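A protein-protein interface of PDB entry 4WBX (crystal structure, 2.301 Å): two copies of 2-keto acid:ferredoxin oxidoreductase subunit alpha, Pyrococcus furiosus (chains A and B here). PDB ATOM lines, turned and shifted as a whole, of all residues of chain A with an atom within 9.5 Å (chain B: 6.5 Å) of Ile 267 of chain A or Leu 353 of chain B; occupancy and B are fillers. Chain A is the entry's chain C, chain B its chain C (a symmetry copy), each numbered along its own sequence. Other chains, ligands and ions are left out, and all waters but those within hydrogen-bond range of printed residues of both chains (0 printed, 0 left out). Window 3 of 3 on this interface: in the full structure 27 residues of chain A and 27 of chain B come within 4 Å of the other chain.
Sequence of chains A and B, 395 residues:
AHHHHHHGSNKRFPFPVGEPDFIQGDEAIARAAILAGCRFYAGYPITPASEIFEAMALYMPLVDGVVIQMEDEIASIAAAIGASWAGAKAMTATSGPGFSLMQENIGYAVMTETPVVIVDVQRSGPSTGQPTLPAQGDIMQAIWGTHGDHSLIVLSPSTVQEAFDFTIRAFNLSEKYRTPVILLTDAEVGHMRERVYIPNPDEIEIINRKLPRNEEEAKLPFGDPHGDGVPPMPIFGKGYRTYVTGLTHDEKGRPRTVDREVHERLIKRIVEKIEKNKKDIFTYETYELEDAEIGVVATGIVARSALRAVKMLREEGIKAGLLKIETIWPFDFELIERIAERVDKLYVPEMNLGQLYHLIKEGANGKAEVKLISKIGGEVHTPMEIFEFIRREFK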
ATOM      1  N   GLY A 107      31.888  38.184  -3.665  1.00  0.00           N
ATOM      2  CA  GLY A 107      32.083  36.750  -3.574  1.00  0.00           C
ATOM      3  C   GLY A 107      33.491  36.434  -3.103  1.00  0.00           C
ATOM      4  O   GLY A 107      33.714  35.583  -2.232  1.00  0.00           O
ATOM      5  N   TYR A 108      34.440  37.164  -3.666  1.00  0.00           N
ATOM      6  CA  TYR A 108      35.835  36.995  -3.317  1.00  0.00           C
ATOM      7  C   TYR A 108      36.100  37.391  -1.860  1.00  0.00           C
ATOM      8  O   TYR A 108      36.874  36.720  -1.161  1.00  0.00           O
ATOM      9  CB  TYR A 108      36.738  37.803  -4.264  1.00  0.00           C
ATOM     10  CG  TYR A 108      38.169  37.727  -3.833  1.00  0.00           C
ATOM     11  CD1 TYR A 108      39.005  36.712  -4.296  1.00  0.00           C
ATOM     12  CD2 TYR A 108      38.682  38.638  -2.914  1.00  0.00           C
ATOM     13  CE1 TYR A 108      40.315  36.621  -3.872  1.00  0.00           C
ATOM     14  CE2 TYR A 108      39.990  38.547  -2.482  1.00  0.00           C
ATOM     15  CZ  TYR A 108      40.797  37.540  -2.964  1.00  0.00           C
ATOM     16  OH  TYR A 108      42.092  37.478  -2.525  1.00  0.00           O
ATOM     17  N   VAL A 110      34.064  37.197   0.482  1.00  0.00           N
ATOM     18  CA  VAL A 110      33.473  36.129   1.291  1.00  0.00           C
ATOM     19  C   VAL A 110      34.456  35.009   1.608  1.00  0.00           C
ATOM     20  O   VAL A 110      34.552  34.580   2.761  1.00  0.00           O
ATOM     21  CB  VAL A 110      32.255  35.485   0.612  1.00  0.00           C
ATOM     22  CG1 VAL A 110      31.886  34.200   1.330  1.00  0.00           C
ATOM     23  CG2 VAL A 110      31.062  36.426   0.606  1.00  0.00           C
ATOM     24  N   MET A 111      35.182  34.541   0.583  1.00  0.00           N
ATOM     25  CA  MET A 111      36.086  33.383   0.706  1.00  0.00           C
ATOM     26  C   MET A 111      37.353  33.687   1.476  1.00  0.00           C
ATOM     27  O   MET A 111      37.921  32.811   2.140  1.00  0.00           O
ATOM     28  CB  MET A 111      36.482  32.853  -0.668  1.00  0.00           C
ATOM     29  CG  MET A 111      35.385  32.088  -1.396  1.00  0.00           C
ATOM     30  SD  MET A 111      36.071  31.134  -2.768  1.00  0.00           S
ATOM     31  CE  MET A 111      36.666  29.689  -1.885  1.00  0.00           C
ATOM     32  N   THR A 112      37.806  34.923   1.334  1.00  0.00           N
ATOM     33  CA  THR A 112      38.982  35.422   2.005  1.00  0.00           C
ATOM     34  C   THR A 112      38.654  35.823   3.438  1.00  0.00           C
ATOM     35  O   THR A 112      39.542  36.208   4.191  1.00  0.00           O
ATOM     36  CB  THR A 112      39.567  36.657   1.248  1.00  0.00           C
ATOM     37  OG1 THR A 112      38.524  37.282   0.483  1.00  0.00           O
ATOM     38  CG2 THR A 112      40.753  36.293   0.295  1.00  0.00           C
ATOM     39  N   GLU A 113      37.380  35.750   3.810  1.00  0.00           N
ATOM     40  CA  GLU A 113      36.953  36.283   5.094  1.00  0.00           C
ATOM     41  C   GLU A 113      37.486  37.698   5.294  1.00  0.00           C
ATOM     42  O   GLU A 113      38.196  37.974   6.279  1.00  0.00           O
ATOM     43  CB  GLU A 113      37.422  35.374   6.219  1.00  0.00           C
ATOM     44  CG  GLU A 113      36.822  33.966   6.146  1.00  0.00           C
ATOM     45  CD  GLU A 113      37.281  33.087   7.285  1.00  0.00           C
ATOM     46  OE1 GLU A 113      38.412  32.560   7.208  1.00  0.00           O
ATOM     47  OE2 GLU A 113      36.516  32.949   8.261  1.00  0.00           O
ATOM     48  N   TRP A 144      21.972  36.251  -2.841  1.00  0.00           N
ATOM     49  CA  TRP A 144      22.389  35.159  -3.712  1.00  0.00           C
ATOM     50  C   TRP A 144      23.189  35.570  -4.961  1.00  0.00           C
ATOM     51  O   TRP A 144      23.365  34.759  -5.872  1.00  0.00           O
ATOM     52  CB  TRP A 144      21.162  34.402  -4.204  1.00  0.00           C
ATOM     53  CG  TRP A 144      20.284  33.733  -3.197  1.00  0.00           C
ATOM     54  CD1 TRP A 144      18.997  34.073  -2.883  1.00  0.00           C
ATOM     55  CD2 TRP A 144      20.581  32.547  -2.449  1.00  0.00           C
ATOM     56  NE1 TRP A 144      18.494  33.198  -1.958  1.00  0.00           N
ATOM     57  CE2 TRP A 144      19.442  32.245  -1.677  1.00  0.00           C
ATOM     58  CE3 TRP A 144      21.708  31.713  -2.348  1.00  0.00           C
ATOM     59  CZ2 TRP A 144      19.392  31.146  -0.808  1.00  0.00           C
ATOM     60  CZ3 TRP A 144      21.659  30.623  -1.482  1.00  0.00           C
ATOM     61  CH2 TRP A 144      20.508  30.351  -0.728  1.00  0.00           C
ATOM     62  N   HIS A 147      28.678  34.139  -6.704  1.00  0.00           N
ATOM     63  CA  HIS A 147      28.801  32.788  -7.228  1.00  0.00           C
ATOM     64  C   HIS A 147      29.204  31.835  -6.096  1.00  0.00           C
ATOM     65  O   HIS A 147      30.011  32.192  -5.224  1.00  0.00           O
ATOM     66  CB  HIS A 147      29.823  32.729  -8.372  1.00  0.00           C
ATOM     67  CG  HIS A 147      30.625  31.458  -8.394  1.00  0.00           C
ATOM     68  ND1 HIS A 147      30.095  30.250  -8.792  1.00  0.00           N
ATOM     69  CD2 HIS A 147      31.910  31.213  -8.036  1.00  0.00           C
ATOM     70  CE1 HIS A 147      31.024  29.308  -8.687  1.00  0.00           C
ATOM     71  NE2 HIS A 147      32.131  29.867  -8.233  1.00  0.00           N
ATOM     72  N   GLY A 148      28.627  30.638  -6.105  1.00  0.00           N
ATOM     73  CA  GLY A 148      29.034  29.588  -5.191  1.00  0.00           C
ATOM     74  C   GLY A 148      28.229  29.486  -3.905  1.00  0.00           C
ATOM     75  O   GLY A 148      27.120  30.007  -3.796  1.00  0.00           O
ATOM     76  N   ASP A 149      28.812  28.791  -2.934  1.00  0.00           N
ATOM     77  CA  ASP A 149      28.264  28.651  -1.591  1.00  0.00           C
ATOM     78  C   ASP A 149      28.962  29.634  -0.705  1.00  0.00           C
ATOM     79  O   ASP A 149      30.185  29.658  -0.644  1.00  0.00           O
ATOM     80  CB  ASP A 149      28.473  27.236  -1.034  1.00  0.00           C
ATOM     81  CG  ASP A 149      27.425  26.267  -1.507  1.00  0.00           C
ATOM     82  OD1 ASP A 149      26.216  26.544  -1.307  1.00  0.00           O
ATOM     83  OD2 ASP A 149      27.824  25.243  -2.103  1.00  0.00           O
ATOM     84  N   HIS A 150      28.184  30.420   0.013  1.00  0.00           N
ATOM     85  CA  HIS A 150      28.731  31.546   0.741  1.00  0.00           C
ATOM     86  C   HIS A 150      27.715  31.915   1.794  1.00  0.00           C
ATOM     87  O   HIS A 150      26.581  31.444   1.758  1.00  0.00           O
ATOM     88  CB  HIS A 150      28.958  32.728  -0.193  1.00  0.00           C
ATOM     89  CG  HIS A 150      27.683  33.206  -0.807  1.00  0.00           C
ATOM     90  ND1 HIS A 150      27.186  32.683  -1.981  1.00  0.00           N
ATOM     91  CD2 HIS A 150      26.749  34.072  -0.355  1.00  0.00           C
ATOM     92  CE1 HIS A 150      26.024  33.248  -2.257  1.00  0.00           C
ATOM     93  NE2 HIS A 150      25.734  34.092  -1.285  1.00  0.00           N
ATOM     94  N   SER A 151      28.117  32.768   2.720  1.00  0.00           N
ATOM     95  CA  SER A 151      27.172  33.394   3.620  1.00  0.00           C
ATOM     96  C   SER A 151      27.700  34.782   3.945  1.00  0.00           C
ATOM     97  O   SER A 151      28.899  34.983   4.200  1.00  0.00           O
ATOM     98  CB  SER A 151      26.963  32.556   4.885  1.00  0.00           C
ATOM     99  OG  SER A 151      25.703  32.845   5.479  1.00  0.00           O
ATOM    100  N   LEU A 266      36.423  24.546   4.998  1.00  0.00           N
ATOM    101  CA  LEU A 266      36.848  25.773   4.325  1.00  0.00           C
ATOM    102  C   LEU A 266      35.613  26.641   4.101  1.00  0.00           C
ATOM    103  O   LEU A 266      35.289  27.501   4.924  1.00  0.00           O
ATOM    104  N   ILE A 267      34.900  26.394   3.005  1.00  0.00           N
ATOM    105  CA  ILE A 267      33.654  27.104   2.769  1.00  0.00           C
ATOM    106  C   ILE A 267      32.496  26.409   3.489  1.00  0.00           C
ATOM    107  O   ILE A 267      31.323  26.723   3.264  1.00  0.00           O
ATOM    108  CB  ILE A 267      33.318  27.227   1.263  1.00  0.00           C
ATOM    109  CG1 ILE A 267      32.764  25.912   0.712  1.00  0.00           C
ATOM    110  CG2 ILE A 267      34.526  27.708   0.463  1.00  0.00           C
ATOM    111  CD1 ILE A 267      32.292  26.009  -0.724  1.00  0.00           C
ATOM    112  N   LYS A 268      32.812  25.460   4.359  1.00  0.00           N
ATOM    113  CA  LYS A 268      31.782  24.864   5.197  1.00  0.00           C
ATOM    114  C   LYS A 268      31.727  25.637   6.499  1.00  0.00           C
ATOM    115  O   LYS A 268      30.666  25.883   7.036  1.00  0.00           O
ATOM    116  CB  LYS A 268      32.063  23.379   5.453  1.00  0.00           C
ATOM    117  N   ARG A 269      32.891  26.029   6.997  1.00  0.00           N
ATOM    118  CA  ARG A 269      32.953  26.807   8.226  1.00  0.00           C
ATOM    119  C   ARG A 269      32.578  28.268   7.965  1.00  0.00           C
ATOM    120  O   ARG A 269      31.911  28.918   8.792  1.00  0.00           O
ATOM    121  CB  ARG A 269      34.333  26.684   8.867  1.00  0.00           C
ATOM    122  CG  ARG A 269      34.522  25.257   9.413  1.00  0.00           C
ATOM    123  CD  ARG A 269      33.249  24.884  10.201  1.00  0.00           C
ATOM    124  NE  ARG A 269      33.097  23.463  10.498  1.00  0.00           N
ATOM    125  CZ  ARG A 269      33.762  22.812  11.445  1.00  0.00           C
ATOM    126  NH1 ARG A 269      34.652  23.452  12.199  1.00  0.00           N
ATOM    127  NH2 ARG A 269      33.535  21.513  11.634  1.00  0.00           N
ATOM    128  N   ILE A 270      32.983  28.773   6.806  1.00  0.00           N
ATOM    129  CA  ILE A 270      32.524  30.074   6.363  1.00  0.00           C
ATOM    130  C   ILE A 270      31.001  30.183   6.449  1.00  0.00           C
ATOM    131  O   ILE A 270      30.480  31.091   7.106  1.00  0.00           O
ATOM    132  CB  ILE A 270      32.988  30.359   4.941  1.00  0.00           C
ATOM    133  CG1 ILE A 270      34.493  30.640   4.948  1.00  0.00           C
ATOM    134  CG2 ILE A 270      32.231  31.544   4.361  1.00  0.00           C
ATOM    135  CD1 ILE A 270      35.039  30.981   3.598  1.00  0.00           C
ATOM    136  N   VAL A 271      30.288  29.261   5.806  1.00  0.00           N
ATOM    137  CA  VAL A 271      28.830  29.330   5.809  1.00  0.00           C
ATOM    138  C   VAL A 271      28.274  29.177   7.223  1.00  0.00           C
ATOM    139  O   VAL A 271      27.265  29.797   7.591  1.00  0.00           O
ATOM    140  CB  VAL A 271      28.220  28.257   4.885  1.00  0.00           C
ATOM    141  CG1 VAL A 271      26.679  28.177   5.034  1.00  0.00           C
ATOM    142  CG2 VAL A 271      28.615  28.539   3.450  1.00  0.00           C
ATOM    143  N   GLU A 272      28.945  28.358   8.022  1.00  0.00           N
ATOM    144  CA  GLU A 272      28.456  28.058   9.358  1.00  0.00           C
ATOM    145  C   GLU A 272      28.749  29.197  10.309  1.00  0.00           C
ATOM    146  O   GLU A 272      28.028  29.394  11.272  1.00  0.00           O
ATOM    147  CB  GLU A 272      29.065  26.756   9.873  1.00  0.00           C
ATOM    148  CG  GLU A 272      28.437  25.537   9.241  1.00  0.00           C
ATOM    149  CD  GLU A 272      29.029  24.242   9.739  1.00  0.00           C
ATOM    150  OE1 GLU A 272      30.118  24.258  10.356  1.00  0.00           O
ATOM    151  OE2 GLU A 272      28.389  23.199   9.509  1.00  0.00           O
ATOM    152  N   LYS A 273      29.822  29.927  10.023  1.00  0.00           N
ATOM    153  CA  LYS A 273      30.202  31.140  10.746  1.00  0.00           C
ATOM    154  C   LYS A 273      28.982  32.039  10.918  1.00  0.00           C
ATOM    155  O   LYS A 273      28.646  32.496  12.017  1.00  0.00           O
ATOM    156  CB  LYS A 273      31.302  31.861   9.974  1.00  0.00           C
ATOM    157  CG  LYS A 273      32.045  32.921  10.723  1.00  0.00           C
ATOM    158  CD  LYS A 273      33.278  33.365   9.936  1.00  0.00           C
ATOM    159  CE  LYS A 273      32.912  33.820   8.514  1.00  0.00           C
ATOM    160  NZ  LYS A 273      33.990  34.618   7.829  1.00  0.00           N
ATOM    161  N   ILE A 274      28.294  32.240   9.804  1.00  0.00           N
ATOM    162  CA  ILE A 274      27.140  33.094   9.762  1.00  0.00           C
ATOM    163  C   ILE A 274      25.897  32.317  10.160  1.00  0.00           C
ATOM    164  O   ILE A 274      25.229  32.683  11.135  1.00  0.00           O
ATOM    165  CB  ILE A 274      26.943  33.716   8.350  1.00  0.00           C
ATOM    166  CG1 ILE A 274      28.197  34.472   7.912  1.00  0.00           C
ATOM    167  CG2 ILE A 274      25.754  34.634   8.340  1.00  0.00           C
ATOM    168  CD1 ILE A 274      28.782  35.334   9.004  1.00  0.00           C
ATOM    169  N   GLU A 275      25.585  31.252   9.422  1.00  0.00           N
ATOM    170  CA  GLU A 275      24.276  30.589   9.559  1.00  0.00           C
ATOM    171  C   GLU A 275      24.042  29.912  10.904  1.00  0.00           C
ATOM    172  O   GLU A 275      22.894  29.724  11.309  1.00  0.00           O
ATOM    173  CB  GLU A 275      24.074  29.571   8.444  1.00  0.00           C
ATOM    174  CG  GLU A 275      23.616  30.206   7.144  1.00  0.00           C
ATOM    175  CD  GLU A 275      22.148  30.610   7.186  1.00  0.00           C
ATOM    176  OE1 GLU A 275      21.747  31.562   6.472  1.00  0.00           O
ATOM    177  OE2 GLU A 275      21.391  29.951   7.926  1.00  0.00           O
ATOM    178  N   TRP A 329      19.609  38.801   6.008  1.00  0.00           N
ATOM    179  CA  TRP A 329      20.350  37.546   5.933  1.00  0.00           C
ATOM    180  C   TRP A 329      21.521  37.591   6.904  1.00  0.00           C
ATOM    181  O   TRP A 329      22.163  38.623   7.043  1.00  0.00           O
ATOM    182  CB  TRP A 329      20.838  37.303   4.504  1.00  0.00           C
ATOM    183  CG  TRP A 329      21.226  35.901   4.256  1.00  0.00           C
ATOM    184  CD1 TRP A 329      22.468  35.347   4.411  1.00  0.00           C
ATOM    185  CD2 TRP A 329      20.365  34.844   3.800  1.00  0.00           C
ATOM    186  NE1 TRP A 329      22.425  34.003   4.088  1.00  0.00           N
ATOM    187  CE2 TRP A 329      21.150  33.677   3.706  1.00  0.00           C
ATOM    188  CE3 TRP A 329      19.005  34.775   3.463  1.00  0.00           C
ATOM    189  CZ2 TRP A 329      20.618  32.453   3.302  1.00  0.00           C
ATOM    190  CZ3 TRP A 329      18.481  33.553   3.057  1.00  0.00           C
ATOM    191  CH2 TRP A 329      19.288  32.410   2.982  1.00  0.00           C
ATOM    192  N   GLY B 137      26.724  25.000  -7.174  1.00  0.00           N
ATOM    193  CA  GLY B 137      26.547  26.216  -6.404  1.00  0.00           C
ATOM    194  C   GLY B 137      26.223  27.534  -7.120  1.00  0.00           C
ATOM    195  O   GLY B 137      26.478  28.601  -6.547  1.00  0.00           O
ATOM    196  N   GLU B 350      21.979  17.841  -3.441  1.00  0.00           N
ATOM    197  CA  GLU B 350      22.643  18.794  -4.334  1.00  0.00           C
ATOM    198  C   GLU B 350      24.125  18.831  -4.038  1.00  0.00           C
ATOM    199  O   GLU B 350      24.560  18.476  -2.940  1.00  0.00           O
ATOM    200  CB  GLU B 350      22.090  20.206  -4.177  1.00  0.00           C
ATOM    201  CG  GLU B 350      20.634  20.310  -3.801  1.00  0.00           C
ATOM    202  CD  GLU B 350      20.204  21.752  -3.561  1.00  0.00           C
ATOM    203  OE1 GLU B 350      20.800  22.674  -4.185  1.00  0.00           O
ATOM    204  OE2 GLU B 350      19.249  21.969  -2.776  1.00  0.00           O
ATOM    205  N   MET B 351      24.906  19.279  -5.008  1.00  0.00           N
ATOM    206  CA  MET B 351      26.306  19.577  -4.730  1.00  0.00           C
ATOM    207  C   MET B 351      26.497  21.073  -4.335  1.00  0.00           C
ATOM    208  O   MET B 351      27.163  21.845  -5.026  1.00  0.00           O
ATOM    209  CB  MET B 351      27.170  19.201  -5.929  1.00  0.00           C
ATOM    210  CG  MET B 351      27.064  17.732  -6.352  1.00  0.00           C
ATOM    211  SD  MET B 351      28.132  17.386  -7.764  1.00  0.00           S
ATOM    212  CE  MET B 351      29.743  17.584  -6.999  1.00  0.00           C
ATOM    213  N   ASN B 352      25.876  21.457  -3.221  1.00  0.00           N
ATOM    214  CA  ASN B 352      25.949  22.802  -2.668  1.00  0.00           C
ATOM    215  C   ASN B 352      25.552  22.734  -1.188  1.00  0.00           C
ATOM    216  O   ASN B 352      25.488  21.639  -0.619  1.00  0.00           O
ATOM    217  CB  ASN B 352      25.054  23.747  -3.451  1.00  0.00           C
ATOM    218  CG  ASN B 352      23.603  23.335  -3.419  1.00  0.00           C
ATOM    219  OD1 ASN B 352      23.073  22.982  -2.367  1.00  0.00           O
ATOM    220  ND2 ASN B 352      22.939  23.390  -4.575  1.00  0.00           N
ATOM    221  N   LEU B 353      25.262  23.864  -0.551  1.00  0.00           N
ATOM    222  CA  LEU B 353      24.801  23.798   0.836  1.00  0.00           C
ATOM    223  C   LEU B 353      23.337  24.130   0.955  1.00  0.00           C
ATOM    224  O   LEU B 353      22.870  24.481   2.026  1.00  0.00           O
ATOM    225  CB  LEU B 353      25.619  24.710   1.743  1.00  0.00           C
ATOM    226  CG  LEU B 353      27.044  24.167   1.894  1.00  0.00           C
ATOM    227  CD1 LEU B 353      27.951  25.021   2.783  1.00  0.00           C
ATOM    228  CD2 LEU B 353      26.980  22.755   2.418  1.00  0.00           C
ATOM    229  N   GLY B 354      22.607  23.993  -0.141  1.00  0.00           N
ATOM    230  CA  GLY B 354      21.169  24.159  -0.113  1.00  0.00           C
ATOM    231  C   GLY B 354      20.741  25.319  -0.982  1.00  0.00           C
ATOM    232  O   GLY B 354      20.944  26.479  -0.621  1.00  0.00           O
ATOM    233  N   GLN B 355      20.158  25.012  -2.135  1.00  0.00           N
ATOM    234  CA  GLN B 355      19.712  26.035  -3.061  1.00  0.00           C
ATOM    235  C   GLN B 355      18.484  25.507  -3.744  1.00  0.00           C
ATOM    236  O   GLN B 355      17.426  26.117  -3.687  1.00  0.00           O
ATOM    237  CB  GLN B 355      20.797  26.386  -4.101  1.00  0.00           C
ATOM    238  CG  GLN B 355      22.114  26.883  -3.511  1.00  0.00           C
ATOM    239  CD  GLN B 355      23.186  27.160  -4.553  1.00  0.00           C
ATOM    240  OE1 GLN B 355      22.927  27.174  -5.767  1.00  0.00           O
ATOM    241  NE2 GLN B 355      24.407  27.383  -4.078  1.00  0.00           N
ATOM    242  N   TYR B 357      17.159  22.932  -2.660  1.00  0.00           N
ATOM    243  CA  TYR B 357      16.449  22.668  -1.412  1.00  0.00           C
ATOM    244  C   TYR B 357      15.416  23.713  -1.030  1.00  0.00           C
ATOM    245  O   TYR B 357      14.287  23.364  -0.664  1.00  0.00           O
ATOM    246  CB  TYR B 357      17.443  22.532  -0.256  1.00  0.00           C
ATOM    247  CG  TYR B 357      16.796  22.730   1.093  1.00  0.00           C
ATOM    248  CD1 TYR B 357      16.143  21.677   1.736  1.00  0.00           C
ATOM    249  CD2 TYR B 357      16.823  23.970   1.727  1.00  0.00           C
ATOM    250  CE1 TYR B 357      15.536  21.858   2.974  1.00  0.00           C
ATOM    251  CE2 TYR B 357      16.217  24.161   2.960  1.00  0.00           C
ATOM    252  CZ  TYR B 357      15.581  23.103   3.577  1.00  0.00           C
ATOM    253  OH  TYR B 357      14.991  23.300   4.802  1.00  0.00           O
ATOM    254  N   HIS B 358      15.817  24.982  -1.076  1.00  0.00           N
ATOM    255  CA  HIS B 358      14.956  26.081  -0.647  1.00  0.00           C
ATOM    256  C   HIS B 358      13.713  26.171  -1.502  1.00  0.00           C
ATOM    257  O   HIS B 358      12.632  26.391  -0.985  1.00  0.00           O
ATOM    258  CB  HIS B 358      15.696  27.420  -0.691  1.00  0.00           C
ATOM    259  CG  HIS B 358      16.783  27.554   0.328  1.00  0.00           C
ATOM    260  ND1 HIS B 358      16.585  28.157   1.551  1.00  0.00           N
ATOM    261  CD2 HIS B 358      18.086  27.183   0.299  1.00  0.00           C
ATOM    262  CE1 HIS B 358      17.715  28.137   2.236  1.00  0.00           C
ATOM    263  NE2 HIS B 358      18.644  27.552   1.499  1.00  0.00           N
ATOM    264  N   LEU B 372      17.993  17.900   2.778  1.00  0.00           N
ATOM    265  CA  LEU B 372      19.054  18.064   1.788  1.00  0.00           C
ATOM    266  C   LEU B 372      20.197  17.077   2.021  1.00  0.00           C
ATOM    267  O   LEU B 372      20.660  16.914   3.151  1.00  0.00           O
ATOM    268  CB  LEU B 372      19.588  19.513   1.812  1.00  0.00           C
ATOM    269  CG  LEU B 372      21.037  19.796   1.349  1.00  0.00           C
ATOM    270  CD1 LEU B 372      21.177  19.833  -0.171  1.00  0.00           C
ATOM    271  CD2 LEU B 372      21.590  21.092   1.955  1.00  0.00           C
ATOM    272  N   SER B 374      23.759  17.065   1.134  1.00  0.00           N
ATOM    273  CA  SER B 374      24.719  17.966   0.556  1.00  0.00           C
ATOM    274  C   SER B 374      26.056  17.305   0.463  1.00  0.00           C
ATOM    275  O   SER B 374      26.641  16.936   1.481  1.00  0.00           O
ATOM    276  CB  SER B 374      24.849  19.234   1.393  1.00  0.00           C
ATOM    277  OG  SER B 374      25.794  19.034   2.429  1.00  0.00           O
ATOM    278  N   LYS B 375      26.568  17.151  -0.743  1.00  0.00           N
ATOM    279  CA  LYS B 375      27.986  16.901  -0.805  1.00  0.00           C
ATOM    280  C   LYS B 375      28.621  17.987  -1.631  1.00  0.00           C
ATOM    281  O   LYS B 375      28.077  18.393  -2.652  1.00  0.00           O
ATOM    282  CB  LYS B 375      28.321  15.534  -1.378  1.00  0.00           C
ATOM    283  CG  LYS B 375      29.828  15.317  -1.377  1.00  0.00           C
ATOM    284  CD  LYS B 375      30.236  14.020  -1.989  1.00  0.00           C
ATOM    285  CE  LYS B 375      29.079  13.077  -2.037  1.00  0.00           C
ATOM    286  NZ  LYS B 375      29.272  12.200  -3.198  1.00  0.00           N
ATOM    287  N   ILE B 376      29.766  18.465  -1.164  1.00  0.00           N
ATOM    288  CA  ILE B 376      30.528  19.487  -1.859  1.00  0.00           C
ATOM    289  C   ILE B 376      32.001  19.131  -1.711  1.00  0.00           C
ATOM    290  O   ILE B 376      32.385  18.418  -0.787  1.00  0.00           O
ATOM    291  CB  ILE B 376      30.257  20.908  -1.294  1.00  0.00           C
ATOM    292  CG1 ILE B 376      30.606  20.971   0.191  1.00  0.00           C
ATOM    293  CG2 ILE B 376      28.797  21.302  -1.463  1.00  0.00           C
ATOM    294  CD1 ILE B 376      31.536  22.084   0.538  1.00  0.00           C
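The backbone NH (N) of Gly 148 of chain A sits at hydrogen-bond distance from the backbone carbonyl oxygen (O) of Gly 137 of chain B, at 3.0 Å. The backbone NH (N) of Leu 353 of chain B lies within hydrogen-bond range of the side-chain carboxylate (OD1) of Asp 149 of chain A (2.9 Å). OD1 of Asp 149 of chain A sits at hydrogen-bond distance from NE2 of Gln 355 of chain B (3.4 Å).
The backbone carbonyl oxygen (O) of Gly 148 of chain A lies within hydrogen-bond range of a ring nitrogen (ND1) of His 150 of chain A (3.2 Å). O of Gly 137 of chain B sits close to NE2 of Gln 355 of chain B. OE1 of Glu 350 of chain B lies close to OD1 of Asn 352 of chain B (2.9 Å). The backbone NH (N) of Gln 355 of chain B sits at hydrogen-bond distance from the side-chain carboxylate (OE1) of Glu 350 of chain B, at 3.2 Å. The backbone NH of Gly 354 of chain B lies within hydrogen-bond range of the side-chain amide oxygen of Asn 352 of chain B (2.5 Å). A ring nitrogen (NE2) of His 358 of chain B sits close to the backbone carbonyl oxygen of Gly 354 of chain B.
Among the printed residues, merely in contact across the chains: Asp 149 of chain A with Asn 352 of chain B (3.1 Å), Val 271 of chain A with Leu 353 of chain B (3.6 Å), Gly 148 of chain A with Gln 355 of chain B (3.8 Å), Ile 267 of chain A with Leu 353 of chain B (3.8 Å) and Trp 144 of chain A with Gly 354 of chain B (3.9 Å).
Ile 267 of chain A touches just one residue of chain B: Leu 353. Leu 353 of chain B touches just these residues of chain A: Asp 149, Ile 267 and Val 271. Of chain A, only Asp 149 (3.1 Å) comes within 4 Å of Asn 352 of chain B. Gly 354 of chain B touches one residue of chain A. Of the printed residues of chain B, Asp 149 of chain A touches Asn 352 (3.1 Å), Leu 353 (2.9 Å) and Gln 355 (3.4 Å). Printed residues of chain B within 4 Å of Val 271 of chain A: Leu 353 (3.6 Å). Glu 350 of chain B touches none of the printed residues of chain A. Ile 274 of chain A touches none of the printed residues of chain B.
Of the 13 printed residues of chain B, 5 touch a printed residue of chain A. Hydrophobic or aromatic side chains of chain B within 4 Å of the printed part of chain A: Leu 353. Hydrophobic or aromatic side chains of chain A that line the printed part of chain B: Trp 144 and Val 271. Among the printed residues, no Asp or Glu carboxylate lies within 4 Å of a Lys or Arg side-chain nitrogen of the other chain.
No position is printed for both chains.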
